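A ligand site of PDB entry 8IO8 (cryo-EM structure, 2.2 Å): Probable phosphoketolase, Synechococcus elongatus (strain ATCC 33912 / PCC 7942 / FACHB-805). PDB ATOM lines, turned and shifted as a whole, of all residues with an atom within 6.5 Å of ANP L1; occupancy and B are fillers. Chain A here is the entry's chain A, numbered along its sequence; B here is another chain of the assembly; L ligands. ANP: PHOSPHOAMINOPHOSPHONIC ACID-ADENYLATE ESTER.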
ATOM      1  N   PRO A 702      19.735 -26.947 -27.405  1.00  0.00           N
ATOM      2  CA  PRO A 702      20.904 -27.628 -27.989  1.00  0.00           C
ATOM      3  C   PRO A 702      21.736 -28.414 -26.990  1.00  0.00           C
ATOM      4  O   PRO A 702      22.361 -29.409 -27.387  1.00  0.00           O
ATOM      5  CB  PRO A 702      21.707 -26.463 -28.588  1.00  0.00           C
ATOM      6  CG  PRO A 702      20.706 -25.403 -28.821  1.00  0.00           C
ATOM      7  CD  PRO A 702      19.735 -25.502 -27.698  1.00  0.00           C
ATOM      8  N   TRP A 703      21.761 -27.981 -25.738  1.00  0.00           N
ATOM      9  CA  TRP A 703      22.557 -28.645 -24.700  1.00  0.00           C
ATOM     10  C   TRP A 703      22.163 -30.110 -24.475  1.00  0.00           C
ATOM     11  O   TRP A 703      22.975 -30.911 -24.007  1.00  0.00           O
ATOM     12  CB  TRP A 703      22.467 -27.881 -23.385  1.00  0.00           C
ATOM     13  CG  TRP A 703      21.119 -27.954 -22.738  1.00  0.00           C
ATOM     14  CD1 TRP A 703      20.122 -27.018 -22.805  1.00  0.00           C
ATOM     15  CD2 TRP A 703      20.620 -29.017 -21.919  1.00  0.00           C
ATOM     16  NE1 TRP A 703      19.029 -27.445 -22.081  1.00  0.00           N
ATOM     17  CE2 TRP A 703      19.310 -28.663 -21.533  1.00  0.00           C
ATOM     18  CE3 TRP A 703      21.142 -30.244 -21.488  1.00  0.00           C
ATOM     19  CZ2 TRP A 703      18.522 -29.486 -20.718  1.00  0.00           C
ATOM     20  CZ3 TRP A 703      20.360 -31.051 -20.687  1.00  0.00           C
ATOM     21  CH2 TRP A 703      19.067 -30.673 -20.309  1.00  0.00           C
ATOM     22  N   LEU A 704      20.930 -30.454 -24.820  1.00  0.00           N
ATOM     23  CA  LEU A 704      20.433 -31.813 -24.634  1.00  0.00           C
ATOM     24  C   LEU A 704      21.139 -32.793 -25.569  1.00  0.00           C
ATOM     25  O   LEU A 704      21.415 -33.930 -25.174  1.00  0.00           O
ATOM     26  CB  LEU A 704      18.924 -31.839 -24.862  1.00  0.00           C
ATOM     27  CG  LEU A 704      18.256 -33.217 -24.780  1.00  0.00           C
ATOM     28  CD1 LEU A 704      18.495 -33.819 -23.414  1.00  0.00           C
ATOM     29  CD2 LEU A 704      16.774 -33.094 -25.069  1.00  0.00           C
ATOM     30  N   HIS A 706      24.158 -32.499 -26.611  1.00  0.00           N
ATOM     31  CA  HIS A 706      25.496 -32.629 -26.050  1.00  0.00           C
ATOM     32  C   HIS A 706      25.475 -33.585 -24.866  1.00  0.00           C
ATOM     33  O   HIS A 706      26.384 -34.394 -24.695  1.00  0.00           O
ATOM     34  CB  HIS A 706      26.021 -31.255 -25.611  1.00  0.00           C
ATOM     35  CG  HIS A 706      26.632 -30.455 -26.721  1.00  0.00           C
ATOM     36  ND1 HIS A 706      27.822 -30.796 -27.319  1.00  0.00           N
ATOM     37  CD2 HIS A 706      26.210 -29.330 -27.349  1.00  0.00           C
ATOM     38  CE1 HIS A 706      28.110 -29.915 -28.260  1.00  0.00           C
ATOM     39  NE2 HIS A 706      27.148 -29.017 -28.296  1.00  0.00           N
ATOM     40  N   LYS A 707      24.421 -33.491 -24.053  1.00  0.00           N
ATOM     41  CA  LYS A 707      24.291 -34.372 -22.894  1.00  0.00           C
ATOM     42  C   LYS A 707      24.197 -35.827 -23.316  1.00  0.00           C
ATOM     43  O   LYS A 707      24.792 -36.708 -22.694  1.00  0.00           O
ATOM     44  CB  LYS A 707      23.062 -33.962 -22.079  1.00  0.00           C
ATOM     45  CG  LYS A 707      22.753 -34.886 -20.922  1.00  0.00           C
ATOM     46  CD  LYS A 707      21.394 -34.573 -20.332  1.00  0.00           C
ATOM     47  CE  LYS A 707      21.039 -35.560 -19.240  1.00  0.00           C
ATOM     48  NZ  LYS A 707      21.140 -36.961 -19.710  1.00  0.00           N
ATOM     49  N   TYR A 710      27.930 -36.930 -25.504  1.00  0.00           N
ATOM     50  CA  TYR A 710      29.173 -36.261 -25.168  1.00  0.00           C
ATOM     51  C   TYR A 710      30.378 -37.181 -25.324  1.00  0.00           C
ATOM     52  O   TYR A 710      31.470 -36.704 -25.652  1.00  0.00           O
ATOM     53  CB  TYR A 710      29.120 -35.701 -23.751  1.00  0.00           C
ATOM     54  CG  TYR A 710      29.197 -36.726 -22.657  1.00  0.00           C
ATOM     55  CD1 TYR A 710      28.068 -37.410 -22.241  1.00  0.00           C
ATOM     56  CD2 TYR A 710      30.401 -37.007 -22.035  1.00  0.00           C
ATOM     57  CE1 TYR A 710      28.137 -38.349 -21.244  1.00  0.00           C
ATOM     58  CE2 TYR A 710      30.473 -37.945 -21.029  1.00  0.00           C
ATOM     59  CZ  TYR A 710      29.348 -38.615 -20.636  1.00  0.00           C
ATOM     60  OH  TYR A 710      29.417 -39.553 -19.640  1.00  0.00           O
ATOM     61  N   HIS A 715      32.497 -36.160 -31.062  1.00  0.00           N
ATOM     62  CA  HIS A 715      31.766 -35.124 -30.356  1.00  0.00           C
ATOM     63  C   HIS A 715      32.409 -33.748 -30.536  1.00  0.00           C
ATOM     64  O   HIS A 715      31.717 -32.730 -30.448  1.00  0.00           O
ATOM     65  CB  HIS A 715      31.666 -35.467 -28.879  1.00  0.00           C
ATOM     66  CG  HIS A 715      30.917 -34.457 -28.057  1.00  0.00           C
ATOM     67  ND1 HIS A 715      31.276 -34.136 -26.771  1.00  0.00           N
ATOM     68  CD2 HIS A 715      29.829 -33.704 -28.348  1.00  0.00           C
ATOM     69  CE1 HIS A 715      30.441 -33.227 -26.298  1.00  0.00           C
ATOM     70  NE2 HIS A 715      29.555 -32.945 -27.240  1.00  0.00           N
ATOM     71  N   LEU A 718      30.606 -31.998 -33.336  1.00  0.00           N
ATOM     72  CA  LEU A 718      29.154 -31.898 -33.237  1.00  0.00           C
ATOM     73  C   LEU A 718      28.766 -30.455 -32.924  1.00  0.00           C
ATOM     74  O   LEU A 718      29.081 -29.936 -31.856  1.00  0.00           O
ATOM     75  CB  LEU A 718      28.629 -32.841 -32.166  1.00  0.00           C
ATOM     76  CG  LEU A 718      27.119 -32.882 -31.962  1.00  0.00           C
ATOM     77  CD1 LEU A 718      26.428 -33.279 -33.241  1.00  0.00           C
ATOM     78  CD2 LEU A 718      26.776 -33.832 -30.844  1.00  0.00           C
ATOM     79  N   HIS A 719      28.082 -29.811 -33.866  1.00  0.00           N
ATOM     80  CA  HIS A 719      27.662 -28.427 -33.731  1.00  0.00           C
ATOM     81  C   HIS A 719      26.143 -28.378 -33.819  1.00  0.00           C
ATOM     82  O   HIS A 719      25.578 -28.644 -34.885  1.00  0.00           O
ATOM     83  CB  HIS A 719      28.315 -27.557 -34.807  1.00  0.00           C
ATOM     84  CG  HIS A 719      29.768 -27.827 -34.974  1.00  0.00           C
ATOM     85  ND1 HIS A 719      30.707 -27.441 -34.040  1.00  0.00           N
ATOM     86  CD2 HIS A 719      30.452 -28.458 -35.949  1.00  0.00           C
ATOM     87  CE1 HIS A 719      31.911 -27.818 -34.448  1.00  0.00           C
ATOM     88  NE2 HIS A 719      31.778 -28.435 -35.605  1.00  0.00           N
ATOM     89  N   VAL A 720      25.497 -28.030 -32.716  1.00  0.00           N
ATOM     90  CA  VAL A 720      24.052 -28.189 -32.554  1.00  0.00           C
ATOM     91  C   VAL A 720      23.405 -26.810 -32.565  1.00  0.00           C
ATOM     92  O   VAL A 720      23.834 -25.908 -31.852  1.00  0.00           O
ATOM     93  CB  VAL A 720      23.709 -28.948 -31.262  1.00  0.00           C
ATOM     94  CG1 VAL A 720      22.222 -29.205 -31.187  1.00  0.00           C
ATOM     95  CG2 VAL A 720      24.476 -30.243 -31.206  1.00  0.00           C
ATOM     96  N   ARG A 721      22.317 -26.700 -33.333  1.00  0.00           N
ATOM     97  CA  ARG A 721      21.524 -25.488 -33.430  1.00  0.00           C
ATOM     98  C   ARG A 721      20.102 -25.869 -33.019  1.00  0.00           C
ATOM     99  O   ARG A 721      19.546 -26.838 -33.539  1.00  0.00           O
ATOM    100  CB  ARG A 721      21.532 -24.945 -34.859  1.00  0.00           C
ATOM    101  CG  ARG A 721      22.924 -24.659 -35.404  1.00  0.00           C
ATOM    102  CD  ARG A 721      23.549 -23.452 -34.728  1.00  0.00           C
ATOM    103  NE  ARG A 721      24.975 -23.337 -35.031  1.00  0.00           N
ATOM    104  CZ  ARG A 721      25.776 -22.414 -34.499  1.00  0.00           C
ATOM    105  NH1 ARG A 721      25.300 -21.533 -33.628  1.00  0.00           N
ATOM    106  NH2 ARG A 721      27.059 -22.387 -34.827  1.00  0.00           N
ATOM    107  N   ASP A 749      26.542 -21.859 -41.271  1.00  0.00           N
ATOM    108  CA  ASP A 749      27.244 -22.715 -40.336  1.00  0.00           C
ATOM    109  C   ASP A 749      28.081 -23.763 -41.051  1.00  0.00           C
ATOM    110  O   ASP A 749      29.190 -24.092 -40.626  1.00  0.00           O
ATOM    111  CB  ASP A 749      26.261 -23.393 -39.386  1.00  0.00           C
ATOM    112  CG  ASP A 749      25.589 -22.409 -38.442  1.00  0.00           C
ATOM    113  OD1 ASP A 749      25.946 -21.211 -38.489  1.00  0.00           O
ATOM    114  OD2 ASP A 749      24.704 -22.824 -37.673  1.00  0.00           O
ATOM    115  N   ARG A 753      32.263 -24.278 -40.860  1.00  0.00           N
ATOM    116  CA  ARG A 753      32.797 -25.553 -40.399  1.00  0.00           C
ATOM    117  C   ARG A 753      33.634 -26.374 -41.383  1.00  0.00           C
ATOM    118  O   ARG A 753      34.563 -27.076 -40.987  1.00  0.00           O
ATOM    119  CB  ARG A 753      31.669 -26.434 -39.855  1.00  0.00           C
ATOM    120  CG  ARG A 753      31.007 -25.891 -38.594  1.00  0.00           C
ATOM    121  CD  ARG A 753      32.036 -25.290 -37.652  1.00  0.00           C
ATOM    122  NE  ARG A 753      31.441 -24.865 -36.390  1.00  0.00           N
ATOM    123  CZ  ARG A 753      30.790 -23.712 -36.218  1.00  0.00           C
ATOM    124  NH1 ARG A 753      30.656 -22.870 -37.226  1.00  0.00           N
ATOM    125  NH2 ARG A 753      30.281 -23.415 -35.027  1.00  0.00           N
ATOM    126  N   GLU B 674      29.341 -15.113 -21.972  1.00  0.00           N
ATOM    127  CA  GLU B 674      27.926 -15.450 -21.964  1.00  0.00           C
ATOM    128  C   GLU B 674      27.122 -14.471 -21.119  1.00  0.00           C
ATOM    129  O   GLU B 674      26.004 -14.094 -21.489  1.00  0.00           O
ATOM    130  CB  GLU B 674      27.724 -16.882 -21.462  1.00  0.00           C
ATOM    131  CG  GLU B 674      28.560 -17.908 -22.189  1.00  0.00           C
ATOM    132  CD  GLU B 674      28.085 -19.323 -21.934  1.00  0.00           C
ATOM    133  OE1 GLU B 674      26.930 -19.489 -21.499  1.00  0.00           O
ATOM    134  OE2 GLU B 674      28.870 -20.266 -22.181  1.00  0.00           O
ATOM    135  N   TRP B 703      25.291 -33.203 -15.180  1.00  0.00           N
ATOM    136  CA  TRP B 703      25.298 -32.633 -16.524  1.00  0.00           C
ATOM    137  C   TRP B 703      25.165 -31.114 -16.541  1.00  0.00           C
ATOM    138  O   TRP B 703      25.602 -30.445 -17.489  1.00  0.00           O
ATOM    139  CB  TRP B 703      24.199 -33.261 -17.383  1.00  0.00           C
ATOM    140  CG  TRP B 703      22.815 -32.892 -16.946  1.00  0.00           C
ATOM    141  CD1 TRP B 703      21.996 -33.591 -16.114  1.00  0.00           C
ATOM    142  CD2 TRP B 703      22.094 -31.712 -17.317  1.00  0.00           C
ATOM    143  NE1 TRP B 703      20.801 -32.935 -15.949  1.00  0.00           N
ATOM    144  CE2 TRP B 703      20.835 -31.771 -16.674  1.00  0.00           C
ATOM    145  CE3 TRP B 703      22.371 -30.614 -18.136  1.00  0.00           C
ATOM    146  CZ2 TRP B 703      19.866 -30.779 -16.819  1.00  0.00           C
ATOM    147  CZ3 TRP B 703      21.414 -29.627 -18.275  1.00  0.00           C
ATOM    148  CH2 TRP B 703      20.171 -29.719 -17.625  1.00  0.00           C
ATOM    149  N   HIS B 706      28.484 -29.358 -16.499  1.00  0.00           N
ATOM    150  CA  HIS B 706      29.084 -29.459 -17.822  1.00  0.00           C
ATOM    151  C   HIS B 706      28.464 -28.418 -18.744  1.00  0.00           C
ATOM    152  O   HIS B 706      29.169 -27.781 -19.538  1.00  0.00           O
ATOM    153  CB  HIS B 706      28.881 -30.864 -18.397  1.00  0.00           C
ATOM    154  CG  HIS B 706      29.956 -31.829 -18.015  1.00  0.00           C
ATOM    155  ND1 HIS B 706      31.254 -31.711 -18.461  1.00  0.00           N
ATOM    156  CD2 HIS B 706      29.928 -32.930 -17.231  1.00  0.00           C
ATOM    157  CE1 HIS B 706      31.977 -32.706 -17.970  1.00  0.00           C
ATOM    158  NE2 HIS B 706      31.197 -33.455 -17.216  1.00  0.00           N
ATOM    159  N   LYS B 707      27.151 -28.239 -18.650  1.00  0.00           N
ATOM    160  CA  LYS B 707      26.459 -27.268 -19.475  1.00  0.00           C
ATOM    161  C   LYS B 707      26.969 -25.851 -19.205  1.00  0.00           C
ATOM    162  O   LYS B 707      27.153 -25.059 -20.134  1.00  0.00           O
ATOM    163  CB  LYS B 707      24.951 -27.346 -19.227  1.00  0.00           C
ATOM    164  CG  LYS B 707      24.161 -26.293 -19.953  1.00  0.00           C
ATOM    165  CD  LYS B 707      22.733 -26.254 -19.440  1.00  0.00           C
ATOM    166  CE  LYS B 707      21.957 -25.128 -20.100  1.00  0.00           C
ATOM    167  NZ  LYS B 707      22.653 -23.829 -19.974  1.00  0.00           N
ATOM    168  N   LEU B 708      27.217 -25.533 -17.929  1.00  0.00           N
ATOM    169  CA  LEU B 708      27.640 -24.181 -17.578  1.00  0.00           C
ATOM    170  C   LEU B 708      29.085 -23.918 -17.961  1.00  0.00           C
ATOM    171  O   LEU B 708      29.409 -22.839 -18.463  1.00  0.00           O
ATOM    172  CB  LEU B 708      27.443 -23.946 -16.078  1.00  0.00           C
ATOM    173  CG  LEU B 708      26.013 -23.980 -15.562  1.00  0.00           C
ATOM    174  CD1 LEU B 708      26.010 -23.871 -14.058  1.00  0.00           C
ATOM    175  CD2 LEU B 708      25.202 -22.868 -16.185  1.00  0.00           C
ATOM    176  N   TYR B 710      31.481 -25.590 -20.085  1.00  0.00           N
ATOM    177  CA  TYR B 710      32.113 -26.342 -21.164  1.00  0.00           C
ATOM    178  C   TYR B 710      33.074 -25.498 -21.984  1.00  0.00           C
ATOM    179  O   TYR B 710      33.933 -26.070 -22.676  1.00  0.00           O
ATOM    180  CB  TYR B 710      31.056 -26.956 -22.083  1.00  0.00           C
ATOM    181  CG  TYR B 710      30.464 -25.974 -23.056  1.00  0.00           C
ATOM    182  CD1 TYR B 710      30.886 -25.931 -24.379  1.00  0.00           C
ATOM    183  CD2 TYR B 710      29.472 -25.096 -22.660  1.00  0.00           C
ATOM    184  CE1 TYR B 710      30.343 -25.043 -25.270  1.00  0.00           C
ATOM    185  CE2 TYR B 710      28.927 -24.194 -23.551  1.00  0.00           C
ATOM    186  CZ  TYR B 710      29.370 -24.170 -24.848  1.00  0.00           C
ATOM    187  OH  TYR B 710      28.819 -23.276 -25.737  1.00  0.00           O
ATOM    188  N   ARG B 711      32.950 -24.180 -21.909  1.00  0.00           N
ATOM    189  CA  ARG B 711      33.815 -23.288 -22.661  1.00  0.00           C
ATOM    190  C   ARG B 711      35.057 -22.857 -21.893  1.00  0.00           C
ATOM    191  O   ARG B 711      35.677 -21.841 -22.208  1.00  0.00           O
ATOM    192  CB  ARG B 711      33.040 -22.051 -23.121  1.00  0.00           C
ATOM    193  CG  ARG B 711      32.125 -22.300 -24.319  1.00  0.00           C
ATOM    194  CD  ARG B 711      31.385 -21.030 -24.719  1.00  0.00           C
ATOM    195  NE  ARG B 711      30.485 -21.263 -25.836  1.00  0.00           N
ATOM    196  CZ  ARG B 711      29.765 -20.316 -26.434  1.00  0.00           C
ATOM    197  NH1 ARG B 711      29.841 -19.057 -26.006  1.00  0.00           N
ATOM    198  NH2 ARG B 711      28.965 -20.621 -27.448  1.00  0.00           N
ATOM    199  N   HIS B 715      38.099 -27.702 -19.086  1.00  0.00           N
ATOM    200  CA  HIS B 715      36.899 -28.535 -19.023  1.00  0.00           C
ATOM    201  C   HIS B 715      37.222 -30.012 -19.223  1.00  0.00           C
ATOM    202  O   HIS B 715      36.479 -30.872 -18.748  1.00  0.00           O
ATOM    203  CB  HIS B 715      35.887 -28.064 -20.064  1.00  0.00           C
ATOM    204  CG  HIS B 715      34.634 -28.869 -20.099  1.00  0.00           C
ATOM    205  ND1 HIS B 715      33.967 -29.163 -21.275  1.00  0.00           N
ATOM    206  CD2 HIS B 715      33.906 -29.442 -19.105  1.00  0.00           C
ATOM    207  CE1 HIS B 715      32.896 -29.880 -20.999  1.00  0.00           C
ATOM    208  NE2 HIS B 715      32.838 -30.070 -19.696  1.00  0.00           N
HETATM  209  PG  ANP L   1      30.506 -23.510 -29.769  1.00  0.00           P
HETATM  210  O1G ANP L   1      31.656 -23.043 -30.604  1.00  0.00           O
HETATM  211  O2G ANP L   1      30.741 -25.019 -29.383  1.00  0.00           O
HETATM  212  O3G ANP L   1      30.424 -22.651 -28.451  1.00  0.00           O
HETATM  213  PB  ANP L   1      28.788 -24.657 -31.628  1.00  0.00           P
HETATM  214  O1B ANP L   1      28.633 -24.213 -33.042  1.00  0.00           O
HETATM  215  O2B ANP L   1      29.992 -25.632 -31.524  1.00  0.00           O
HETATM  216  N3B ANP L   1      29.057 -23.342 -30.644  1.00  0.00           N
HETATM  217  PA  ANP L   1      27.530 -26.311 -29.899  1.00  0.00           P
HETATM  218  O1A ANP L   1      28.922 -26.601 -29.502  1.00  0.00           O
HETATM  219  O2A ANP L   1      26.715 -27.547 -30.271  1.00  0.00           O
HETATM  220  O3A ANP L   1      27.487 -25.378 -31.175  1.00  0.00           O
HETATM  221  O5' ANP L   1      26.832 -25.493 -28.744  1.00  0.00           O
HETATM  222  C5' ANP L   1      25.410 -25.584 -28.518  1.00  0.00           C
HETATM  223  C4' ANP L   1      25.125 -25.557 -27.038  1.00  0.00           C
HETATM  224  O4' ANP L   1      25.508 -26.802 -26.443  1.00  0.00           O
HETATM  225  C3' ANP L   1      25.881 -24.517 -26.224  1.00  0.00           C
HETATM  226  O3' ANP L   1      25.197 -23.267 -26.247  1.00  0.00           O
HETATM  227  C2' ANP L   1      25.916 -25.118 -24.810  1.00  0.00           C
HETATM  228  O2' ANP L   1      24.958 -24.537 -23.938  1.00  0.00           O
HETATM  229  C1' ANP L   1      25.588 -26.607 -25.041  1.00  0.00           C
HETATM  230  N9  ANP L   1      26.564 -27.540 -24.492  1.00  0.00           N
HETATM  231  C8  ANP L   1      26.474 -28.228 -23.304  1.00  0.00           C
HETATM  232  N7  ANP L   1      27.500 -29.005 -23.062  1.00  0.00           N
HETATM  233  C5  ANP L   1      28.324 -28.823 -24.152  1.00  0.00           C
HETATM  234  C6  ANP L   1      29.573 -29.373 -24.505  1.00  0.00           C
HETATM  235  N6  ANP L   1      30.231 -30.255 -23.745  1.00  0.00           N
HETATM  236  N1  ANP L   1      30.120 -28.984 -25.677  1.00  0.00           N
HETATM  237  C2  ANP L   1      29.464 -28.117 -26.437  1.00  0.00           C
HETATM  238  N3  ANP L   1      28.289 -27.530 -26.212  1.00  0.00           N
HETATM  239  C4  ANP L   1      27.770 -27.929 -25.050  1.00  0.00           C
HETATM  240  PG  ANP L   2      33.381 -39.751 -17.890  1.00  0.00           P
HETATM  241  O1G ANP L   2      34.696 -40.494 -17.721  1.00  0.00           O
HETATM  242  O2G ANP L   2      33.531 -38.370 -18.466  1.00  0.00           O
HETATM  243  O3G ANP L   2      32.306 -40.580 -18.544  1.00  0.00           O
HETATM  244  PB  ANP L   2      33.629 -38.334 -15.221  1.00  0.00           P
HETATM  245  O1B ANP L   2      34.718 -37.670 -16.030  1.00  0.00           O
HETATM  246  O2B ANP L   2      34.014 -39.047 -13.941  1.00  0.00           O
HETATM  247  N3B ANP L   2      32.818 -39.492 -16.256  1.00  0.00           N
HETATM  248  PA  ANP L   2      32.010 -36.169 -15.927  1.00  0.00           P
HETATM  249  O1A ANP L   2      32.889 -36.276 -17.155  1.00  0.00           O
HETATM  250  O2A ANP L   2      31.801 -34.825 -15.271  1.00  0.00           O
HETATM  251  O3A ANP L   2      32.573 -37.187 -14.811  1.00  0.00           O
HETATM  252  O5' ANP L   2      30.570 -36.797 -16.273  1.00  0.00           O
HETATM  253  C5' ANP L   2      29.587 -36.961 -15.261  1.00  0.00           C
HETATM  254  C4' ANP L   2      28.195 -36.782 -15.857  1.00  0.00           C
HETATM  255  O4' ANP L   2      28.159 -35.570 -16.621  1.00  0.00           O
HETATM  256  C3' ANP L   2      27.843 -37.926 -16.784  1.00  0.00           C
HETATM  257  O3' ANP L   2      26.713 -38.641 -16.269  1.00  0.00           O
HETATM  258  C2' ANP L   2      27.578 -37.306 -18.151  1.00  0.00           C
HETATM  259  O2' ANP L   2      26.244 -37.564 -18.632  1.00  0.00           O
HETATM  260  C1' ANP L   2      27.781 -35.815 -17.978  1.00  0.00           C
HETATM  261  N9  ANP L   2      28.854 -35.345 -18.889  1.00  0.00           N
HETATM  262  C8  ANP L   2      30.162 -35.629 -18.772  1.00  0.00           C
HETATM  263  N7  ANP L   2      30.882 -35.050 -19.764  1.00  0.00           N
HETATM  264  C5  ANP L   2      30.025 -34.365 -20.543  1.00  0.00           C
HETATM  265  C6  ANP L   2      30.119 -33.533 -21.771  1.00  0.00           C
HETATM  266  N6  ANP L   2      31.308 -33.301 -22.363  1.00  0.00           N
HETATM  267  N1  ANP L   2      28.977 -33.014 -22.257  1.00  0.00           N
HETATM  268  C2  ANP L   2      27.783 -33.233 -21.675  1.00  0.00           C
HETATM  269  N3  ANP L   2      27.619 -33.982 -20.562  1.00  0.00           N
HETATM  270  C4  ANP L   2      28.685 -34.565 -19.968  1.00  0.00           C
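A ring nitrogen (NE2) of His 706 of chain A is in hydrogen-bond range of an oxygen (O2A) of ANP L1 (2.5 Å).
NH2 of Arg 711 of chain B lies within salt-bridge range of O3G of ANP L1, at 2.7 Å.
The guanidinium group (NH2) of Arg 753 lies within salt-bridge range of an oxygen (O1B) of ANP L1 (2.7 Å).
N of Val 720 lies within hydrogen-bond range of O2A of ANP L1 (2.8 Å).
The guanidinium group (NH2) of Arg 721 is in salt-bridge range of an oxygen (O1B) of ANP L1.
ND1 of His 719 sits at hydrogen-bond distance from O2B of ANP L1 (3.2 Å).
O3G of ANP L1 lies within hydrogen-bond range of OH of Tyr 710 of chain B (3.2 Å).
NE2 of His 706 of chain B sits at hydrogen-bond distance from O2A of ANP L2, at 2.5 Å.
The side-chain hydroxyl (OH) of Tyr 710 of chain A is in hydrogen-bond range of an oxygen (O3G) of ANP L2 (3.3 Å).
A nitrogen (N6) of ANP L1 is in hydrogen-bond range of a nitrogen (N1) of ANP L2, at 3.4 Å.
A ring nitrogen (NE2) of His 715 of chain A sits at hydrogen-bond distance from a ring nitrogen (ND1) of His 706 of chain A.
NE of Arg 711 of chain B lies within hydrogen-bond range of OH of Tyr 710 of chain B.
OD2 of Asp 749 is in salt-bridge range of NE of Arg 721, at 2.7 Å.
The backbone carbonyl oxygen (O) of Tyr 710 of chain B sits close to a ring nitrogen (ND1) of His 715 of chain B (3.4 Å).
NE2 of His 715 of chain B sits at hydrogen-bond distance from ND1 of His 706 of chain B (2.6 Å).
A ring nitrogen (ND1) of His 715 of chain A is in hydrogen-bond range of the backbone carbonyl oxygen (O) of Tyr 710 of chain A.
Pro 702 touches ANP L1 (CB to C5', 3.8 Å).
Trp 703 of chain A touches ANP L1 (CA to C1', 3.7 Å).
CE1 of His 715 of chain A touches N6 of ANP L1 (3.9 Å).
Leu 718 touches ANP L1.
CA of Lys 707 of chain B touches C8 of ANP L1 (3.9 Å).
CE1 of His 715 of chain B touches N6 of ANP L1 (3.8 Å).
Hydrophobic or aromatic side chains that line ANP L1: Pro 702, Trp 703 of chain A, His 706 of chain A, His 715 of chain A, His 719, Val 720, Tyr 710 of chain B and His 715 of chain B.
Of the 21 residues printed, 13 come within 4 Å of ANP L1.
The nearest printed residue that does not touch ANP L1 is His 706 of chain B (4.1 Å).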
